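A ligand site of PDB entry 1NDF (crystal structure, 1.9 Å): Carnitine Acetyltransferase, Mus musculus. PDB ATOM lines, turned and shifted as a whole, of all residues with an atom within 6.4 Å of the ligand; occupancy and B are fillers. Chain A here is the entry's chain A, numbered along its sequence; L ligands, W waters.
OH of Tyr 423 is in hydrogen-bond range of O2 of the ligand, at 2.6 Å. O2 of the ligand lies within hydrogen-bond range of OG of Ser 425. O1 of the ligand lies within hydrogen-bond range of OG1 of Thr 436 (2.6 Å). An oxygen (O3) of the ligand is in hydrogen-bond range of a ring nitrogen (NE2) of His 314, 2.7 Å away.
O of Tyr 423 sits at hydrogen-bond distance from N of Thr 524, 2.8 Å away. OH of Tyr 423 lies within hydrogen-bond range of NH2 of Arg 489. The backbone NH (N) of Ser 425 lies within hydrogen-bond range of the backbone carbonyl oxygen (O) of Thr 524, 3.1 Å away. The guanidinium group of Arg 489 is in hydrogen-bond range of the side-chain hydroxyl of Thr 436 (3.0 Å). A ring nitrogen (ND1) of His 314 lies within hydrogen-bond range of the side-chain hydroxyl (OH) of Tyr 78 (3.3 Å). The guanidinium group (NH2) of Arg 435 sits at hydrogen-bond distance from the backbone carbonyl oxygen (O) of His 314, at 3.3 Å. ND1 of His 314 is in hydrogen-bond range of O of Ala 317. The guanidinium group of Arg 435 is in salt-bridge range of the side-chain carboxylate of Glu 318, at 2.6 Å.
CZ2 of Trp 73 touches O1 of the ligand, at 3.6 Å. OH of Tyr 78 touches O1 of the ligand, at 3.9 Å. Glu 318 touches the ligand. OG of Ser 523 touches C7 of the ligand (3.3 Å). Thr 524 touches the ligand. CE2 of Phe 537 touches C6 of the ligand, 3.5 Å away. Val 540 touches the ligand (CG1 to C7, 3.9 Å). Hydrophobic or aromatic side chains that line the ligand: Trp 73, His 314, Tyr 423, Phe 537 and Val 540. 11 residues have an atom within 4 Å of the ligand: Trp 73, Tyr 78, His 314, Glu 318, Tyr 423, Ser 425, Thr 436, Ser 523, Thr 524, Phe 537 and Val 540. The nearest printed residue that does not touch the ligand is Arg 489 (4.03 Å).
Water W1 bridges an oxygen (O3) of the ligand and the side-chain hydroxyl (OG) of Ser 525. Water W3 lies within hydrogen-bond range of OH of Tyr 78 (2.6 Å), OE2 of Glu 318 (2.7 Å), O1 of the ligand (2.8 Å) and NE1 of Trp 73 (2.8 Å). Water W4 lies within hydrogen-bond range of OH of Tyr 423 (3.0 Å) and O1 of the ligand (3.4 Å).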
ATOM      1  N   TRP A  73      31.805 -29.929   9.585  1.00  0.00           N
ATOM      2  CA  TRP A  73      30.739 -28.934   9.466  1.00  0.00           C
ATOM      3  C   TRP A  73      29.485 -29.360  10.220  1.00  0.00           C
ATOM      4  O   TRP A  73      28.931 -28.579  10.990  1.00  0.00           O
ATOM      5  CB  TRP A  73      30.409 -28.672   7.992  1.00  0.00           C
ATOM      6  CG  TRP A  73      29.333 -27.635   7.800  1.00  0.00           C
ATOM      7  CD1 TRP A  73      28.075 -27.835   7.299  1.00  0.00           C
ATOM      8  CD2 TRP A  73      29.401 -26.241   8.167  1.00  0.00           C
ATOM      9  NE1 TRP A  73      27.359 -26.655   7.327  1.00  0.00           N
ATOM     10  CE2 TRP A  73      28.148 -25.671   7.859  1.00  0.00           C
ATOM     11  CE3 TRP A  73      30.405 -25.436   8.727  1.00  0.00           C
ATOM     12  CZ2 TRP A  73      27.867 -24.318   8.089  1.00  0.00           C
ATOM     13  CZ3 TRP A  73      30.124 -24.083   8.957  1.00  0.00           C
ATOM     14  CH2 TRP A  73      28.865 -23.544   8.641  1.00  0.00           C
ATOM     15  N   ALA A  77      28.571 -26.859  13.113  1.00  0.00           N
ATOM     16  CA  ALA A  77      27.409 -26.040  12.831  1.00  0.00           C
ATOM     17  C   ALA A  77      26.140 -26.490  13.525  1.00  0.00           C
ATOM     18  O   ALA A  77      25.298 -25.659  13.862  1.00  0.00           O
ATOM     19  CB  ALA A  77      27.170 -25.997  11.323  1.00  0.00           C
ATOM     20  N   TYR A  78      25.999 -27.794  13.749  1.00  0.00           N
ATOM     21  CA  TYR A  78      24.761 -28.293  14.335  1.00  0.00           C
ATOM     22  C   TYR A  78      24.820 -29.214  15.555  1.00  0.00           C
ATOM     23  O   TYR A  78      24.263 -28.894  16.601  1.00  0.00           O
ATOM     24  CB  TYR A  78      23.936 -28.978  13.248  1.00  0.00           C
ATOM     25  CG  TYR A  78      23.756 -28.126  12.022  1.00  0.00           C
ATOM     26  CD1 TYR A  78      24.482 -28.365  10.858  1.00  0.00           C
ATOM     27  CD2 TYR A  78      22.897 -27.026  12.041  1.00  0.00           C
ATOM     28  CE1 TYR A  78      24.363 -27.539   9.741  1.00  0.00           C
ATOM     29  CE2 TYR A  78      22.759 -26.196  10.936  1.00  0.00           C
ATOM     30  CZ  TYR A  78      23.502 -26.454   9.792  1.00  0.00           C
ATOM     31  OH  TYR A  78      23.368 -25.609   8.704  1.00  0.00           O
ATOM     32  N   SER A  89      17.886 -22.439  15.175  1.00  0.00           N
ATOM     33  CA  SER A  89      18.473 -23.317  14.171  1.00  0.00           C
ATOM     34  C   SER A  89      17.528 -23.796  13.073  1.00  0.00           C
ATOM     35  O   SER A  89      17.861 -23.705  11.896  1.00  0.00           O
ATOM     36  CB  SER A  89      19.109 -24.528  14.880  1.00  0.00           C
ATOM     37  OG  SER A  89      19.669 -25.441  13.949  1.00  0.00           O
ATOM     38  N   PRO A  91      14.809 -23.689  10.418  1.00  0.00           N
ATOM     39  CA  PRO A  91      14.106 -22.679   9.610  1.00  0.00           C
ATOM     40  C   PRO A  91      12.626 -22.989   9.442  1.00  0.00           C
ATOM     41  O   PRO A  91      12.231 -24.161   9.377  1.00  0.00           O
ATOM     42  CB  PRO A  91      14.836 -22.733   8.273  1.00  0.00           C
ATOM     43  CG  PRO A  91      16.193 -23.282   8.626  1.00  0.00           C
ATOM     44  CD  PRO A  91      15.835 -24.357   9.612  1.00  0.00           C
ATOM     45  N   TYR A 312      11.844 -27.283   9.476  1.00  0.00           N
ATOM     46  CA  TYR A 312      12.723 -28.435   9.342  1.00  0.00           C
ATOM     47  C   TYR A 312      13.963 -28.302  10.193  1.00  0.00           C
ATOM     48  O   TYR A 312      14.449 -27.202  10.450  1.00  0.00           O
ATOM     49  CB  TYR A 312      13.088 -28.650   7.874  1.00  0.00           C
ATOM     50  CG  TYR A 312      13.951 -27.578   7.241  1.00  0.00           C
ATOM     51  CD1 TYR A 312      15.339 -27.701   7.211  1.00  0.00           C
ATOM     52  CD2 TYR A 312      13.379 -26.464   6.631  1.00  0.00           C
ATOM     53  CE1 TYR A 312      16.142 -26.736   6.583  1.00  0.00           C
ATOM     54  CE2 TYR A 312      14.170 -25.501   5.995  1.00  0.00           C
ATOM     55  CZ  TYR A 312      15.546 -25.649   5.977  1.00  0.00           C
ATOM     56  OH  TYR A 312      16.330 -24.709   5.345  1.00  0.00           O
ATOM     57  N   HIS A 314      17.662 -28.376  10.749  1.00  0.00           N
ATOM     58  CA  HIS A 314      18.818 -28.085   9.897  1.00  0.00           C
ATOM     59  C   HIS A 314      19.981 -29.069   9.793  1.00  0.00           C
ATOM     60  O   HIS A 314      20.676 -29.080   8.776  1.00  0.00           O
ATOM     61  CB  HIS A 314      19.373 -26.705  10.266  1.00  0.00           C
ATOM     62  CG  HIS A 314      19.703 -25.863   9.082  1.00  0.00           C
ATOM     63  ND1 HIS A 314      20.216 -26.385   7.917  1.00  0.00           N
ATOM     64  CD2 HIS A 314      19.584 -24.526   8.874  1.00  0.00           C
ATOM     65  CE1 HIS A 314      20.388 -25.423   7.034  1.00  0.00           C
ATOM     66  NE2 HIS A 314      20.013 -24.283   7.590  1.00  0.00           N
ATOM     67  N   ALA A 317      19.421 -31.088   6.484  1.00  0.00           N
ATOM     68  CA  ALA A 317      19.554 -30.573   5.122  1.00  0.00           C
ATOM     69  C   ALA A 317      19.667 -29.065   4.946  1.00  0.00           C
ATOM     70  O   ALA A 317      19.916 -28.324   5.896  1.00  0.00           O
ATOM     71  CB  ALA A 317      18.395 -31.093   4.264  1.00  0.00           C
ATOM     72  N   GLU A 318      19.482 -28.647   3.699  1.00  0.00           N
ATOM     73  CA  GLU A 318      19.560 -27.258   3.302  1.00  0.00           C
ATOM     74  C   GLU A 318      18.226 -26.823   2.681  1.00  0.00           C
ATOM     75  O   GLU A 318      17.332 -27.655   2.500  1.00  0.00           O
ATOM     76  CB  GLU A 318      20.675 -27.080   2.274  1.00  0.00           C
ATOM     77  CG  GLU A 318      22.046 -27.570   2.742  1.00  0.00           C
ATOM     78  CD  GLU A 318      22.506 -26.841   3.984  1.00  0.00           C
ATOM     79  OE1 GLU A 318      22.093 -25.680   4.170  1.00  0.00           O
ATOM     80  OE2 GLU A 318      23.288 -27.408   4.766  1.00  0.00           O
ATOM     81  N   GLY A 319      18.110 -25.541   2.357  1.00  0.00           N
ATOM     82  CA  GLY A 319      16.880 -25.034   1.779  1.00  0.00           C
ATOM     83  C   GLY A 319      16.500 -25.621   0.418  1.00  0.00           C
ATOM     84  O   GLY A 319      15.382 -26.110   0.266  1.00  0.00           O
ATOM     85  N   TYR A 423      26.828 -12.556   6.405  1.00  0.00           N
ATOM     86  CA  TYR A 423      26.843 -13.938   5.926  1.00  0.00           C
ATOM     87  C   TYR A 423      25.746 -14.211   4.905  1.00  0.00           C
ATOM     88  O   TYR A 423      24.593 -13.862   5.123  1.00  0.00           O
ATOM     89  CB  TYR A 423      26.627 -14.872   7.121  1.00  0.00           C
ATOM     90  CG  TYR A 423      26.644 -16.357   6.796  1.00  0.00           C
ATOM     91  CD1 TYR A 423      27.695 -17.159   7.237  1.00  0.00           C
ATOM     92  CD2 TYR A 423      25.600 -16.965   6.084  1.00  0.00           C
ATOM     93  CE1 TYR A 423      27.713 -18.529   6.978  1.00  0.00           C
ATOM     94  CE2 TYR A 423      25.612 -18.330   5.821  1.00  0.00           C
ATOM     95  CZ  TYR A 423      26.676 -19.107   6.274  1.00  0.00           C
ATOM     96  OH  TYR A 423      26.713 -20.452   6.019  1.00  0.00           O
ATOM     97  N   GLU A 424      26.108 -14.823   3.784  1.00  0.00           N
ATOM     98  CA  GLU A 424      25.095 -15.239   2.808  1.00  0.00           C
ATOM     99  C   GLU A 424      25.437 -16.677   2.436  1.00  0.00           C
ATOM    100  O   GLU A 424      26.568 -16.971   2.081  1.00  0.00           O
ATOM    101  CB  GLU A 424      25.081 -14.401   1.532  1.00  0.00           C
ATOM    102  CG  GLU A 424      23.934 -14.904   0.624  1.00  0.00           C
ATOM    103  CD  GLU A 424      23.968 -14.401  -0.804  1.00  0.00           C
ATOM    104  OE1 GLU A 424      24.936 -13.716  -1.200  1.00  0.00           O
ATOM    105  OE2 GLU A 424      23.012 -14.722  -1.536  1.00  0.00           O
ATOM    106  N   SER A 425      24.449 -17.563   2.512  1.00  0.00           N
ATOM    107  CA  SER A 425      24.662 -18.971   2.169  1.00  0.00           C
ATOM    108  C   SER A 425      25.031 -19.178   0.705  1.00  0.00           C
ATOM    109  O   SER A 425      24.386 -18.601  -0.191  1.00  0.00           O
ATOM    110  CB  SER A 425      23.385 -19.775   2.442  1.00  0.00           C
ATOM    111  OG  SER A 425      22.996 -19.715   3.798  1.00  0.00           O
ATOM    112  N   ALA A 426      26.044 -19.996   0.457  1.00  0.00           N
ATOM    113  CA  ALA A 426      26.463 -20.346  -0.900  1.00  0.00           C
ATOM    114  C   ALA A 426      26.413 -21.871  -0.974  1.00  0.00           C
ATOM    115  O   ALA A 426      26.960 -22.547  -0.096  1.00  0.00           O
ATOM    116  CB  ALA A 426      27.871 -19.861  -1.172  1.00  0.00           C
ATOM    117  N   ARG A 435      27.829 -29.013   1.099  1.00  0.00           N
ATOM    118  CA  ARG A 435      26.746 -28.363   1.830  1.00  0.00           C
ATOM    119  C   ARG A 435      26.803 -26.864   1.484  1.00  0.00           C
ATOM    120  O   ARG A 435      26.251 -26.439   0.468  1.00  0.00           O
ATOM    121  CB  ARG A 435      26.888 -28.535   3.351  1.00  0.00           C
ATOM    122  CG  ARG A 435      26.716 -29.967   3.885  1.00  0.00           C
ATOM    123  CD  ARG A 435      25.266 -30.462   3.828  1.00  0.00           C
ATOM    124  NE  ARG A 435      24.346 -29.752   4.710  1.00  0.00           N
ATOM    125  CZ  ARG A 435      24.044 -30.098   5.964  1.00  0.00           C
ATOM    126  NH1 ARG A 435      24.616 -31.160   6.522  1.00  0.00           N
ATOM    127  NH2 ARG A 435      23.145 -29.402   6.653  1.00  0.00           N
ATOM    128  N   THR A 436      27.507 -26.090   2.302  1.00  0.00           N
ATOM    129  CA  THR A 436      27.584 -24.640   2.081  1.00  0.00           C
ATOM    130  C   THR A 436      28.936 -24.012   2.396  1.00  0.00           C
ATOM    131  O   THR A 436      29.820 -24.641   2.971  1.00  0.00           O
ATOM    132  CB  THR A 436      26.536 -23.884   2.959  1.00  0.00           C
ATOM    133  OG1 THR A 436      26.855 -24.075   4.352  1.00  0.00           O
ATOM    134  CG2 THR A 436      25.136 -24.393   2.703  1.00  0.00           C
ATOM    135  N   ASP A 437      29.088 -22.752   1.979  1.00  0.00           N
ATOM    136  CA  ASP A 437      30.263 -21.951   2.289  1.00  0.00           C
ATOM    137  C   ASP A 437      29.682 -20.550   2.475  1.00  0.00           C
ATOM    138  O   ASP A 437      28.483 -20.341   2.305  1.00  0.00           O
ATOM    139  CB  ASP A 437      31.323 -21.941   1.188  1.00  0.00           C
ATOM    140  CG  ASP A 437      32.744 -21.671   1.745  1.00  0.00           C
ATOM    141  OD1 ASP A 437      32.892 -20.945   2.759  1.00  0.00           O
ATOM    142  OD2 ASP A 437      33.726 -22.186   1.150  1.00  0.00           O
ATOM    143  N   ARG A 489      34.964 -21.694   5.135  1.00  0.00           N
ATOM    144  CA  ARG A 489      35.045 -23.079   5.577  1.00  0.00           C
ATOM    145  C   ARG A 489      36.511 -23.484   5.627  1.00  0.00           C
ATOM    146  O   ARG A 489      36.931 -24.287   6.474  1.00  0.00           O
ATOM    147  CB  ARG A 489      34.269 -23.980   4.620  1.00  0.00           C
ATOM    148  CG  ARG A 489      32.789 -23.679   4.570  1.00  0.00           C
ATOM    149  CD  ARG A 489      32.059 -24.029   5.870  1.00  0.00           C
ATOM    150  NE  ARG A 489      30.641 -23.692   5.732  1.00  0.00           N
ATOM    151  CZ  ARG A 489      30.173 -22.454   5.798  1.00  0.00           C
ATOM    152  NH1 ARG A 489      31.001 -21.441   6.035  1.00  0.00           N
ATOM    153  NH2 ARG A 489      28.883 -22.211   5.561  1.00  0.00           N
ATOM    154  N   SER A 523      22.727 -12.276   8.952  1.00  0.00           N
ATOM    155  CA  SER A 523      22.843 -13.682   8.535  1.00  0.00           C
ATOM    156  C   SER A 523      21.725 -13.858   7.516  1.00  0.00           C
ATOM    157  O   SER A 523      20.552 -13.732   7.854  1.00  0.00           O
ATOM    158  CB  SER A 523      22.628 -14.623   9.718  1.00  0.00           C
ATOM    159  OG  SER A 523      22.708 -15.977   9.261  1.00  0.00           O
ATOM    160  N   THR A 524      22.104 -14.190   6.291  1.00  0.00           N
ATOM    161  CA  THR A 524      21.132 -14.285   5.200  1.00  0.00           C
ATOM    162  C   THR A 524      21.268 -15.482   4.274  1.00  0.00           C
ATOM    163  O   THR A 524      22.269 -16.184   4.276  1.00  0.00           O
ATOM    164  CB  THR A 524      21.264 -13.049   4.309  1.00  0.00           C
ATOM    165  OG1 THR A 524      22.431 -13.204   3.492  1.00  0.00           O
ATOM    166  CG2 THR A 524      21.453 -11.805   5.140  1.00  0.00           C
ATOM    167  N   SER A 525      20.236 -15.673   3.464  1.00  0.00           N
ATOM    168  CA  SER A 525      20.204 -16.730   2.464  1.00  0.00           C
ATOM    169  C   SER A 525      19.069 -16.477   1.475  1.00  0.00           C
ATOM    170  O   SER A 525      18.036 -15.918   1.815  1.00  0.00           O
ATOM    171  CB  SER A 525      20.006 -18.105   3.110  1.00  0.00           C
ATOM    172  OG  SER A 525      18.710 -18.211   3.669  1.00  0.00           O
ATOM    173  N   PHE A 537      14.306 -17.484   9.817  1.00  0.00           N
ATOM    174  CA  PHE A 537      15.068 -18.054  10.923  1.00  0.00           C
ATOM    175  C   PHE A 537      15.546 -16.947  11.838  1.00  0.00           C
ATOM    176  O   PHE A 537      15.559 -15.781  11.460  1.00  0.00           O
ATOM    177  CB  PHE A 537      16.250 -18.875  10.375  1.00  0.00           C
ATOM    178  CG  PHE A 537      17.047 -18.163   9.319  1.00  0.00           C
ATOM    179  CD1 PHE A 537      17.953 -17.173   9.664  1.00  0.00           C
ATOM    180  CD2 PHE A 537      16.901 -18.486   7.971  1.00  0.00           C
ATOM    181  CE1 PHE A 537      18.707 -16.500   8.682  1.00  0.00           C
ATOM    182  CE2 PHE A 537      17.629 -17.832   6.982  1.00  0.00           C
ATOM    183  CZ  PHE A 537      18.539 -16.827   7.343  1.00  0.00           C
ATOM    184  N   GLY A 538      15.922 -17.318  13.059  1.00  0.00           N
ATOM    185  CA  GLY A 538      16.389 -16.322  14.010  1.00  0.00           C
ATOM    186  C   GLY A 538      17.790 -15.837  13.697  1.00  0.00           C
ATOM    187  O   GLY A 538      18.543 -16.513  13.000  1.00  0.00           O
ATOM    188  N   VAL A 540      21.779 -14.961  14.154  1.00  0.00           N
ATOM    189  CA  VAL A 540      22.796 -15.837  14.730  1.00  0.00           C
ATOM    190  C   VAL A 540      23.555 -15.196  15.875  1.00  0.00           C
ATOM    191  O   VAL A 540      24.342 -15.854  16.563  1.00  0.00           O
ATOM    192  CB  VAL A 540      23.781 -16.342  13.645  1.00  0.00           C
ATOM    193  CG1 VAL A 540      23.019 -17.101  12.587  1.00  0.00           C
ATOM    194  CG2 VAL A 540      24.538 -15.184  13.028  1.00  0.00           C
HETATM  195  C1  LIG L   1      24.160 -22.479   5.767  1.00  0.00           C
HETATM  196  O1  LIG L   1      25.043 -23.306   6.094  1.00  0.00           O
HETATM  197  O2  LIG L   1      24.425 -21.381   5.229  1.00  0.00           O
HETATM  198  C2  LIG L   1      22.707 -22.794   6.096  1.00  0.00           C
HETATM  199  C3  LIG L   1      21.883 -21.541   6.438  1.00  0.00           C
HETATM  200  O3  LIG L   1      20.501 -21.900   6.458  1.00  0.00           O
HETATM  201  C4  LIG L   1      22.297 -21.026   7.833  1.00  0.00           C
HETATM  202  N1  LIG L   1      21.701 -19.710   8.104  1.00  0.00           N
HETATM  203  C5  LIG L   1      22.042 -18.767   7.028  1.00  0.00           C
HETATM  204  C6  LIG L   1      20.247 -19.826   8.211  1.00  0.00           C
HETATM  205  C7  LIG L   1      22.237 -19.204   9.361  1.00  0.00           C
HETATM  206  O   HOH W   1      18.865 -21.027   4.552  1.00  0.00           O
HETATM  207  O   HOH W   2      19.628 -21.583  11.099  1.00  0.00           O
HETATM  208  O   HOH W   3      24.740 -26.021   6.526  1.00  0.00           O
HETATM  209  O   HOH W   4      25.853 -21.331   8.705  1.00  0.00           O
